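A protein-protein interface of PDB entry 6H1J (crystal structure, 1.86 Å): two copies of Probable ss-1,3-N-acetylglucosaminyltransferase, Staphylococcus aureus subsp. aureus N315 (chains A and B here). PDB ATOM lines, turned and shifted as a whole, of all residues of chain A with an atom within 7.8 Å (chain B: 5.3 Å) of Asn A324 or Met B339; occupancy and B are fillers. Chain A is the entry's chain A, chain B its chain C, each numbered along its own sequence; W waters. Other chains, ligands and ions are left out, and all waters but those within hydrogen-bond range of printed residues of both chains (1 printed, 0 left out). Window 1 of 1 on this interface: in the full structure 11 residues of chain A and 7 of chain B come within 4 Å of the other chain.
The side-chain amide oxygen (OD1) of Asn B289 sits at hydrogen-bond distance from the side-chain amide nitrogen (ND2) of Asn A324 (2.9 Å).
NZ of Lys B343 sits at hydrogen-bond distance from OD1 of Asn A324 (2.9 Å).
The side-chain amide nitrogen (ND2) of Asn B289 is in hydrogen-bond range of the backbone carbonyl oxygen (O) of Met B339 (3.1 Å).
OD1 of Asp B334 lies close to N of Leu B336 (3.3 Å).
The side-chain amide oxygen (OD1) of Asn A324 lies close to the backbone carbonyl oxygen (O) of Gln A321 (3.3 Å).
OE2 of Glu A328 sits at hydrogen-bond distance from NE2 of Gln A332 (2.7 Å).
Among the printed residues, merely in contact across the chains: Asn A324 with Met B339 (3.4 Å), Leu A325 with Ile B340 (3.5 Å), Leu A325 with Leu B336 (3.6 Å), Ala A329 with Leu B336 (3.7 Å), Gln A332 with Leu B336 (3.7 Å), Leu A325 with Lys B343 (3.7 Å), Leu A325 with Met B339 (3.8 Å), Gln A321 with Asn B289 (3.8 Å) and Glu A328 with Leu B336 (3.97 Å).
Lys A326 touches none of the printed residues of chain B.
Printed residues of chain A within 4 Å of Asn B289: Gln A321 (3.8 Å) and Asn A324 (2.9 Å).
Met B339 touches two residues of chain A.
Of the printed residues of chain A, Ile B340 touches Leu A325 (3.5 Å).
Of the printed residues of chain A, Lys B343 touches Asn A324 and Leu A325.
The nearest residue of chain A that does not touch Met B339 is Glu A328 (4.5 Å).
The nearest printed residue of chain B that does not touch Gln A321 is Lys B343 (5.0 Å).
Of the 19 printed residues of chain A, 6 touch a printed residue of chain B.
Of the 12 printed residues of chain B, 5 touch a printed residue of chain A.
Printed residues of chain B that touch a printed residue of chain A: Asn B289, Leu B336, Met B339, Ile B340 and Lys B343.
Hydrophobic or aromatic side chains of chain B within 4 Å of the printed part of chain A: Leu B336, Met B339 and Ile B340.
Among the printed residues, 11 pairs touch across the chains.
Among the printed residues, no Asp or Glu carboxylate lies within 4 Å of a Lys or Arg side-chain nitrogen of the other chain.
Position printed for both chains: 341.
Water W1 lies within hydrogen-bond range of OE1 of Gln A321 (2.8 Å) and NZ of Lys B343 (3.3 Å).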
ATOM      1  N   LEU A 279      -2.138 -19.420   8.344  1.00  0.00           N
ATOM      2  CA  LEU A 279      -2.040 -20.442   7.299  1.00  0.00           C
ATOM      3  C   LEU A 279      -2.907 -21.648   7.664  1.00  0.00           C
ATOM      4  O   LEU A 279      -3.416 -22.309   6.769  1.00  0.00           O
ATOM      5  CB  LEU A 279      -0.573 -20.857   7.088  1.00  0.00           C
ATOM      6  CG  LEU A 279       0.311 -19.777   6.454  1.00  0.00           C
ATOM      7  CD1 LEU A 279       1.766 -20.200   6.404  1.00  0.00           C
ATOM      8  CD2 LEU A 279      -0.152 -19.390   5.060  1.00  0.00           C
ATOM      9  N   ASP A 316       9.815 -15.523  10.024  1.00  0.00           N
ATOM     10  CA  ASP A 316       9.581 -16.748   9.260  1.00  0.00           C
ATOM     11  C   ASP A 316      10.174 -17.976   9.960  1.00  0.00           C
ATOM     12  O   ASP A 316       9.611 -19.050   9.852  1.00  0.00           O
ATOM     13  CB  ASP A 316      10.105 -16.654   7.826  1.00  0.00           C
ATOM     14  CG  ASP A 316       9.327 -15.698   6.927  1.00  0.00           C
ATOM     15  OD1 ASP A 316       8.326 -15.044   7.415  1.00  0.00           O
ATOM     16  OD2 ASP A 316       9.725 -15.596   5.746  1.00  0.00           O
ATOM     17  N   VAL A 319       7.633 -19.938  12.020  1.00  0.00           N
ATOM     18  CA  VAL A 319       6.543 -20.618  11.342  1.00  0.00           C
ATOM     19  C   VAL A 319       6.875 -22.104  11.248  1.00  0.00           C
ATOM     20  O   VAL A 319       7.988 -22.459  10.900  1.00  0.00           O
ATOM     21  CB  VAL A 319       6.320 -20.051   9.936  1.00  0.00           C
ATOM     22  CG1 VAL A 319       5.213 -20.810   9.207  1.00  0.00           C
ATOM     23  CG2 VAL A 319       6.049 -18.554   9.994  1.00  0.00           C
ATOM     24  N   THR A 320       5.887 -22.955  11.511  1.00  0.00           N
ATOM     25  CA  THR A 320       6.023 -24.422  11.434  1.00  0.00           C
ATOM     26  C   THR A 320       6.559 -24.821  10.047  1.00  0.00           C
ATOM     27  O   THR A 320       6.083 -24.328   9.033  1.00  0.00           O
ATOM     28  CB  THR A 320       4.669 -25.076  11.751  1.00  0.00           C
ATOM     29  OG1 THR A 320       4.243 -24.604  13.037  1.00  0.00           O
ATOM     30  CG2 THR A 320       4.708 -26.579  11.785  1.00  0.00           C
ATOM     31  N   GLN A 321       7.519 -25.748  10.032  1.00  0.00           N
ATOM     32  CA  GLN A 321       8.377 -26.070   8.865  1.00  0.00           C
ATOM     33  C   GLN A 321       7.520 -26.511   7.657  1.00  0.00           C
ATOM     34  O   GLN A 321       7.812 -26.141   6.530  1.00  0.00           O
ATOM     35  CB  GLN A 321       9.423 -27.092   9.332  1.00  0.00           C
ATOM     36  CG  GLN A 321      10.251 -27.770   8.241  1.00  0.00           C
ATOM     37  CD  GLN A 321      11.047 -26.834   7.358  1.00  0.00           C
ATOM     38  OE1 GLN A 321      11.186 -27.045   6.143  1.00  0.00           O
ATOM     39  NE2 GLN A 321      11.602 -25.801   7.968  1.00  0.00           N
ATOM     40  N   ILE A 322       6.447 -27.274   7.884  1.00  0.00           N
ATOM     41  CA  ILE A 322       5.640 -27.809   6.753  1.00  0.00           C
ATOM     42  C   ILE A 322       5.078 -26.691   5.866  1.00  0.00           C
ATOM     43  O   ILE A 322       4.679 -26.983   4.729  1.00  0.00           O
ATOM     44  CB  ILE A 322       4.494 -28.726   7.218  1.00  0.00           C
ATOM     45  CG1 ILE A 322       3.611 -28.050   8.264  1.00  0.00           C
ATOM     46  CG2 ILE A 322       5.042 -30.068   7.672  1.00  0.00           C
ATOM     47  CD1 ILE A 322       2.244 -28.657   8.391  1.00  0.00           C
ATOM     48  N   PHE A 323       4.986 -25.465   6.396  1.00  0.00           N
ATOM     49  CA  PHE A 323       4.417 -24.358   5.708  1.00  0.00           C
ATOM     50  C   PHE A 323       5.478 -23.499   5.020  1.00  0.00           C
ATOM     51  O   PHE A 323       5.124 -22.442   4.495  1.00  0.00           O
ATOM     52  CB  PHE A 323       3.622 -23.463   6.660  1.00  0.00           C
ATOM     53  CG  PHE A 323       2.344 -24.077   7.172  1.00  0.00           C
ATOM     54  CD1 PHE A 323       1.299 -24.361   6.306  1.00  0.00           C
ATOM     55  CD2 PHE A 323       2.194 -24.398   8.517  1.00  0.00           C
ATOM     56  CE1 PHE A 323       0.122 -24.933   6.773  1.00  0.00           C
ATOM     57  CE2 PHE A 323       1.025 -24.986   8.980  1.00  0.00           C
ATOM     58  CZ  PHE A 323      -0.017 -25.239   8.111  1.00  0.00           C
ATOM     59  N   ASN A 324       6.736 -23.959   4.980  1.00  0.00           N
ATOM     60  CA  ASN A 324       7.859 -23.172   4.448  1.00  0.00           C
ATOM     61  C   ASN A 324       7.574 -22.733   2.997  1.00  0.00           C
ATOM     62  O   ASN A 324       7.741 -21.562   2.619  1.00  0.00           O
ATOM     63  CB  ASN A 324       9.183 -23.948   4.557  1.00  0.00           C
ATOM     64  CG  ASN A 324       9.378 -25.117   3.587  1.00  0.00           C
ATOM     65  OD1 ASN A 324       8.473 -25.947   3.347  1.00  0.00           O
ATOM     66  ND2 ASN A 324      10.592 -25.236   3.052  1.00  0.00           N
ATOM     67  N   LEU A 325       7.184 -23.700   2.169  1.00  0.00           N
ATOM     68  CA  LEU A 325       6.974 -23.448   0.755  1.00  0.00           C
ATOM     69  C   LEU A 325       5.732 -22.562   0.563  1.00  0.00           C
ATOM     70  O   LEU A 325       5.779 -21.565  -0.191  1.00  0.00           O
ATOM     71  CB  LEU A 325       6.887 -24.788   0.020  1.00  0.00           C
ATOM     72  CG  LEU A 325       6.346 -24.731  -1.405  1.00  0.00           C
ATOM     73  CD1 LEU A 325       7.260 -23.927  -2.308  1.00  0.00           C
ATOM     74  CD2 LEU A 325       6.114 -26.132  -1.938  1.00  0.00           C
ATOM     75  N   LYS A 326       4.630 -22.871   1.248  1.00  0.00           N
ATOM     76  CA  LYS A 326       3.423 -22.042   1.081  1.00  0.00           C
ATOM     77  C   LYS A 326       3.683 -20.565   1.410  1.00  0.00           C
ATOM     78  O   LYS A 326       3.236 -19.683   0.695  1.00  0.00           O
ATOM     79  CB  LYS A 326       2.239 -22.563   1.890  1.00  0.00           C
ATOM     80  CG  LYS A 326       0.961 -21.773   1.657  1.00  0.00           C
ATOM     81  CD  LYS A 326      -0.272 -22.589   1.851  1.00  0.00           C
ATOM     82  CE  LYS A 326      -1.534 -21.766   1.694  1.00  0.00           C
ATOM     83  NZ  LYS A 326      -2.728 -22.577   2.024  1.00  0.00           N
ATOM     84  N   LEU A 327       4.375 -20.295   2.517  1.00  0.00           N
ATOM     85  CA  LEU A 327       4.674 -18.945   2.946  1.00  0.00           C
ATOM     86  C   LEU A 327       5.574 -18.247   1.913  1.00  0.00           C
ATOM     87  O   LEU A 327       5.358 -17.075   1.574  1.00  0.00           O
ATOM     88  CB  LEU A 327       5.337 -19.011   4.331  1.00  0.00           C
ATOM     89  CG  LEU A 327       5.789 -17.684   4.946  1.00  0.00           C
ATOM     90  CD1 LEU A 327       4.633 -16.738   5.160  1.00  0.00           C
ATOM     91  CD2 LEU A 327       6.530 -17.913   6.254  1.00  0.00           C
ATOM     92  N   GLU A 328       6.588 -18.964   1.407  1.00  0.00           N
ATOM     93  CA  GLU A 328       7.491 -18.353   0.450  1.00  0.00           C
ATOM     94  C   GLU A 328       6.735 -18.072  -0.849  1.00  0.00           C
ATOM     95  O   GLU A 328       6.939 -17.010  -1.451  1.00  0.00           O
ATOM     96  CB  GLU A 328       8.751 -19.196   0.218  1.00  0.00           C
ATOM     97  CG  GLU A 328       9.824 -18.438  -0.546  1.00  0.00           C
ATOM     98  CD  GLU A 328      10.221 -17.090   0.038  1.00  0.00           C
ATOM     99  OE1 GLU A 328      10.459 -17.049   1.262  1.00  0.00           O
ATOM    100  OE2 GLU A 328      10.252 -16.068  -0.720  1.00  0.00           O
ATOM    101  N   ALA A 329       5.865 -19.010  -1.260  1.00  0.00           N
ATOM    102  CA  ALA A 329       5.004 -18.825  -2.441  1.00  0.00           C
ATOM    103  C   ALA A 329       4.190 -17.533  -2.323  1.00  0.00           C
ATOM    104  O   ALA A 329       4.089 -16.756  -3.275  1.00  0.00           O
ATOM    105  CB  ALA A 329       4.107 -20.024  -2.631  1.00  0.00           C
ATOM    106  N   ILE A 330       3.618 -17.316  -1.136  1.00  0.00           N
ATOM    107  CA  ILE A 330       2.835 -16.123  -0.861  1.00  0.00           C
ATOM    108  C   ILE A 330       3.740 -14.878  -0.927  1.00  0.00           C
ATOM    109  O   ILE A 330       3.392 -13.897  -1.592  1.00  0.00           O
ATOM    110  CB  ILE A 330       2.068 -16.282   0.467  1.00  0.00           C
ATOM    111  CG1 ILE A 330       1.021 -17.393   0.360  1.00  0.00           C
ATOM    112  CG2 ILE A 330       1.453 -14.967   0.899  1.00  0.00           C
ATOM    113  CD1 ILE A 330       0.516 -17.907   1.699  1.00  0.00           C
ATOM    114  N   ARG A 331       4.912 -14.914  -0.277  1.00  0.00           N
ATOM    115  CA  ARG A 331       5.867 -13.799  -0.375  1.00  0.00           C
ATOM    116  C   ARG A 331       6.212 -13.485  -1.837  1.00  0.00           C
ATOM    117  O   ARG A 331       6.372 -12.347  -2.167  1.00  0.00           O
ATOM    118  CB  ARG A 331       7.143 -14.074   0.418  1.00  0.00           C
ATOM    119  CG  ARG A 331       6.982 -13.912   1.925  1.00  0.00           C
ATOM    120  CD  ARG A 331       8.304 -13.880   2.662  1.00  0.00           C
ATOM    121  NE  ARG A 331       8.171 -13.765   4.116  1.00  0.00           N
ATOM    122  CZ  ARG A 331       7.881 -12.643   4.779  1.00  0.00           C
ATOM    123  NH1 ARG A 331       7.722 -11.491   4.139  1.00  0.00           N
ATOM    124  NH2 ARG A 331       7.800 -12.689   6.102  1.00  0.00           N
ATOM    125  N   GLN A 332       6.383 -14.510  -2.684  1.00  0.00           N
ATOM    126  CA  GLN A 332       6.766 -14.327  -4.095  1.00  0.00           C
ATOM    127  C   GLN A 332       5.539 -13.992  -4.965  1.00  0.00           C
ATOM    128  O   GLN A 332       5.675 -13.723  -6.141  1.00  0.00           O
ATOM    129  CB  GLN A 332       7.407 -15.604  -4.633  1.00  0.00           C
ATOM    130  CG  GLN A 332       8.731 -16.015  -3.979  1.00  0.00           C
ATOM    131  CD  GLN A 332       9.794 -14.954  -4.097  1.00  0.00           C
ATOM    132  OE1 GLN A 332       9.827 -14.189  -5.055  1.00  0.00           O
ATOM    133  NE2 GLN A 332      10.661 -14.878  -3.098  1.00  0.00           N
ATOM    134  N   ALA A 341       1.907 -26.006  -3.327  1.00  0.00           N
ATOM    135  CA  ALA A 341       2.129 -26.100  -1.895  1.00  0.00           C
ATOM    136  C   ALA A 341       0.914 -26.750  -1.209  1.00  0.00           C
ATOM    137  O   ALA A 341       1.090 -27.601  -0.346  1.00  0.00           O
ATOM    138  CB  ALA A 341       2.417 -24.742  -1.332  1.00  0.00           C
ATOM    139  N   LEU A 344       0.766 -30.502  -1.791  1.00  0.00           N
ATOM    140  CA  LEU A 344       1.761 -31.260  -0.998  1.00  0.00           C
ATOM    141  C   LEU A 344       1.440 -31.243   0.501  1.00  0.00           C
ATOM    142  O   LEU A 344       1.942 -32.093   1.223  1.00  0.00           O
ATOM    143  CB  LEU A 344       3.154 -30.683  -1.227  1.00  0.00           C
ATOM    144  CG  LEU A 344       3.652 -30.796  -2.660  1.00  0.00           C
ATOM    145  CD1 LEU A 344       4.943 -30.030  -2.846  1.00  0.00           C
ATOM    146  CD2 LEU A 344       3.823 -32.247  -3.025  1.00  0.00           C
ATOM    147  N   LEU A 345       0.643 -30.272   0.966  1.00  0.00           N
ATOM    148  CA  LEU A 345       0.190 -30.268   2.368  1.00  0.00           C
ATOM    149  C   LEU A 345      -0.935 -31.294   2.543  1.00  0.00           C
ATOM    150  O   LEU A 345      -1.415 -31.924   1.604  1.00  0.00           O
ATOM    151  CB  LEU A 345      -0.298 -28.874   2.762  1.00  0.00           C
ATOM    152  CG  LEU A 345       0.797 -27.852   3.032  1.00  0.00           C
ATOM    153  CD1 LEU A 345       0.253 -26.442   2.870  1.00  0.00           C
ATOM    154  CD2 LEU A 345       1.391 -28.055   4.416  1.00  0.00           C
ATOM    155  OXT LEU A 345      -1.406 -31.514   3.653  1.00  0.00           O
ATOM    156  N   ALA B 288      17.744 -25.574  -0.532  1.00  0.00           N
ATOM    157  CA  ALA B 288      16.486 -24.840  -0.851  1.00  0.00           C
ATOM    158  C   ALA B 288      15.490 -24.850   0.325  1.00  0.00           C
ATOM    159  O   ALA B 288      14.909 -23.815   0.621  1.00  0.00           O
ATOM    160  CB  ALA B 288      15.861 -25.367  -2.122  1.00  0.00           C
ATOM    161  N   ASN B 289      15.354 -25.980   1.038  1.00  0.00           N
ATOM    162  CA  ASN B 289      14.416 -26.109   2.154  1.00  0.00           C
ATOM    163  C   ASN B 289      15.141 -26.017   3.512  1.00  0.00           C
ATOM    164  O   ASN B 289      14.569 -26.389   4.524  1.00  0.00           O
ATOM    165  CB  ASN B 289      13.664 -27.436   2.090  1.00  0.00           C
ATOM    166  CG  ASN B 289      12.738 -27.484   0.901  1.00  0.00           C
ATOM    167  OD1 ASN B 289      11.818 -26.675   0.806  1.00  0.00           O
ATOM    168  ND2 ASN B 289      12.977 -28.407  -0.010  1.00  0.00           N
ATOM    169  N   ASP B 334      14.997 -20.610 -10.215  1.00  0.00           N
ATOM    170  CA  ASP B 334      13.652 -20.547  -9.605  1.00  0.00           C
ATOM    171  C   ASP B 334      13.649 -21.297  -8.265  1.00  0.00           C
ATOM    172  O   ASP B 334      13.511 -22.549  -8.235  1.00  0.00           O
ATOM    173  CB  ASP B 334      12.620 -21.133 -10.562  1.00  0.00           C
ATOM    174  CG  ASP B 334      11.169 -20.927 -10.152  1.00  0.00           C
ATOM    175  OD1 ASP B 334      10.824 -21.185  -8.980  1.00  0.00           O
ATOM    176  OD2 ASP B 334      10.388 -20.542 -11.028  1.00  0.00           O
ATOM    177  N   LEU B 335      13.735 -20.534  -7.171  1.00  0.00           N
ATOM    178  CA  LEU B 335      13.962 -21.095  -5.843  1.00  0.00           C
ATOM    179  C   LEU B 335      12.767 -21.963  -5.429  1.00  0.00           C
ATOM    180  O   LEU B 335      12.937 -23.015  -4.816  1.00  0.00           O
ATOM    181  CB  LEU B 335      14.188 -19.953  -4.844  1.00  0.00           C
ATOM    182  CG  LEU B 335      14.359 -20.365  -3.382  1.00  0.00           C
ATOM    183  CD1 LEU B 335      15.533 -21.310  -3.201  1.00  0.00           C
ATOM    184  CD2 LEU B 335      14.543 -19.143  -2.493  1.00  0.00           C
ATOM    185  N   LEU B 336      11.553 -21.498  -5.753  1.00  0.00           N
ATOM    186  CA  LEU B 336      10.347 -22.203  -5.333  1.00  0.00           C
ATOM    187  C   LEU B 336      10.356 -23.594  -5.979  1.00  0.00           C
ATOM    188  O   LEU B 336      10.001 -24.597  -5.334  1.00  0.00           O
ATOM    189  CB  LEU B 336       9.115 -21.391  -5.744  1.00  0.00           C
ATOM    190  CG  LEU B 336       8.797 -20.201  -4.845  1.00  0.00           C
ATOM    191  CD1 LEU B 336       7.774 -19.298  -5.492  1.00  0.00           C
ATOM    192  CD2 LEU B 336       8.321 -20.654  -3.479  1.00  0.00           C
ATOM    193  N   ALA B 337      10.785 -23.635  -7.244  1.00  0.00           N
ATOM    194  CA  ALA B 337      10.808 -24.888  -8.012  1.00  0.00           C
ATOM    195  C   ALA B 337      11.890 -25.832  -7.460  1.00  0.00           C
ATOM    196  O   ALA B 337      11.667 -27.026  -7.403  1.00  0.00           O
ATOM    197  CB  ALA B 337      10.976 -24.626  -9.481  1.00  0.00           C
ATOM    198  N   VAL B 338      13.026 -25.299  -7.009  1.00  0.00           N
ATOM    199  CA  VAL B 338      14.015 -26.140  -6.350  1.00  0.00           C
ATOM    200  C   VAL B 338      13.469 -26.698  -5.035  1.00  0.00           C
ATOM    201  O   VAL B 338      13.713 -27.874  -4.718  1.00  0.00           O
ATOM    202  CB  VAL B 338      15.356 -25.433  -6.117  1.00  0.00           C
ATOM    203  CG1 VAL B 338      16.366 -26.419  -5.569  1.00  0.00           C
ATOM    204  CG2 VAL B 338      15.880 -24.765  -7.378  1.00  0.00           C
ATOM    205  N   MET B 339      12.748 -25.867  -4.269  1.00  0.00           N
ATOM    206  CA  MET B 339      12.181 -26.298  -3.023  1.00  0.00           C
ATOM    207  C   MET B 339      11.236 -27.474  -3.268  1.00  0.00           C
ATOM    208  O   MET B 339      11.266 -28.485  -2.544  1.00  0.00           O
ATOM    209  CB  MET B 339      11.394 -25.165  -2.343  1.00  0.00           C
ATOM    210  CG  MET B 339      12.273 -24.050  -1.818  1.00  0.00           C
ATOM    211  SD  MET B 339      11.369 -22.622  -1.206  1.00  0.00           S
ATOM    212  CE  MET B 339      10.702 -23.318   0.302  1.00  0.00           C
ATOM    213  N   ILE B 340      10.365 -27.300  -4.270  1.00  0.00           N
ATOM    214  CA  ILE B 340       9.400 -28.298  -4.642  1.00  0.00           C
ATOM    215  C   ILE B 340      10.127 -29.558  -5.138  1.00  0.00           C
ATOM    216  O   ILE B 340       9.746 -30.671  -4.744  1.00  0.00           O
ATOM    217  CB  ILE B 340       8.426 -27.753  -5.712  1.00  0.00           C
ATOM    218  CG1 ILE B 340       7.523 -26.649  -5.146  1.00  0.00           C
ATOM    219  CG2 ILE B 340       7.600 -28.877  -6.329  1.00  0.00           C
ATOM    220  CD1 ILE B 340       7.050 -25.648  -6.184  1.00  0.00           C
ATOM    221  N   ALA B 341      11.128 -29.384  -6.006  1.00  0.00           N
ATOM    222  CA  ALA B 341      11.883 -30.529  -6.554  1.00  0.00           C
ATOM    223  C   ALA B 341      12.415 -31.378  -5.390  1.00  0.00           C
ATOM    224  O   ALA B 341      12.224 -32.596  -5.405  1.00  0.00           O
ATOM    225  CB  ALA B 341      12.989 -30.055  -7.466  1.00  0.00           C
ATOM    226  N   ASP B 342      12.961 -30.715  -4.340  1.00  0.00           N
ATOM    227  CA  ASP B 342      13.550 -31.415  -3.235  1.00  0.00           C
ATOM    228  C   ASP B 342      12.476 -32.140  -2.439  1.00  0.00           C
ATOM    229  O   ASP B 342      12.750 -33.213  -1.944  1.00  0.00           O
ATOM    230  CB  ASP B 342      14.388 -30.519  -2.324  1.00  0.00           C
ATOM    231  CG  ASP B 342      15.812 -30.303  -2.809  1.00  0.00           C
ATOM    232  OD1 ASP B 342      16.283 -31.109  -3.647  1.00  0.00           O
ATOM    233  OD2 ASP B 342      16.446 -29.333  -2.355  1.00  0.00           O
ATOM    234  N   LYS B 343      11.278 -31.551  -2.301  1.00  0.00           N
ATOM    235  CA  LYS B 343      10.215 -32.208  -1.558  1.00  0.00           C
ATOM    236  C   LYS B 343       9.757 -33.484  -2.274  1.00  0.00           C
ATOM    237  O   LYS B 343       9.312 -34.415  -1.657  1.00  0.00           O
ATOM    238  CB  LYS B 343       9.037 -31.257  -1.336  1.00  0.00           C
ATOM    239  CG  LYS B 343       9.243 -30.244  -0.216  1.00  0.00           C
ATOM    240  CD  LYS B 343       8.170 -29.215  -0.175  1.00  0.00           C
ATOM    241  CE  LYS B 343       8.463 -28.101   0.796  1.00  0.00           C
ATOM    242  NZ  LYS B 343       8.552 -28.612   2.186  1.00  0.00           N
HETATM  243  O   HOH W   1       9.084 -28.786   5.470  1.00  0.00           O
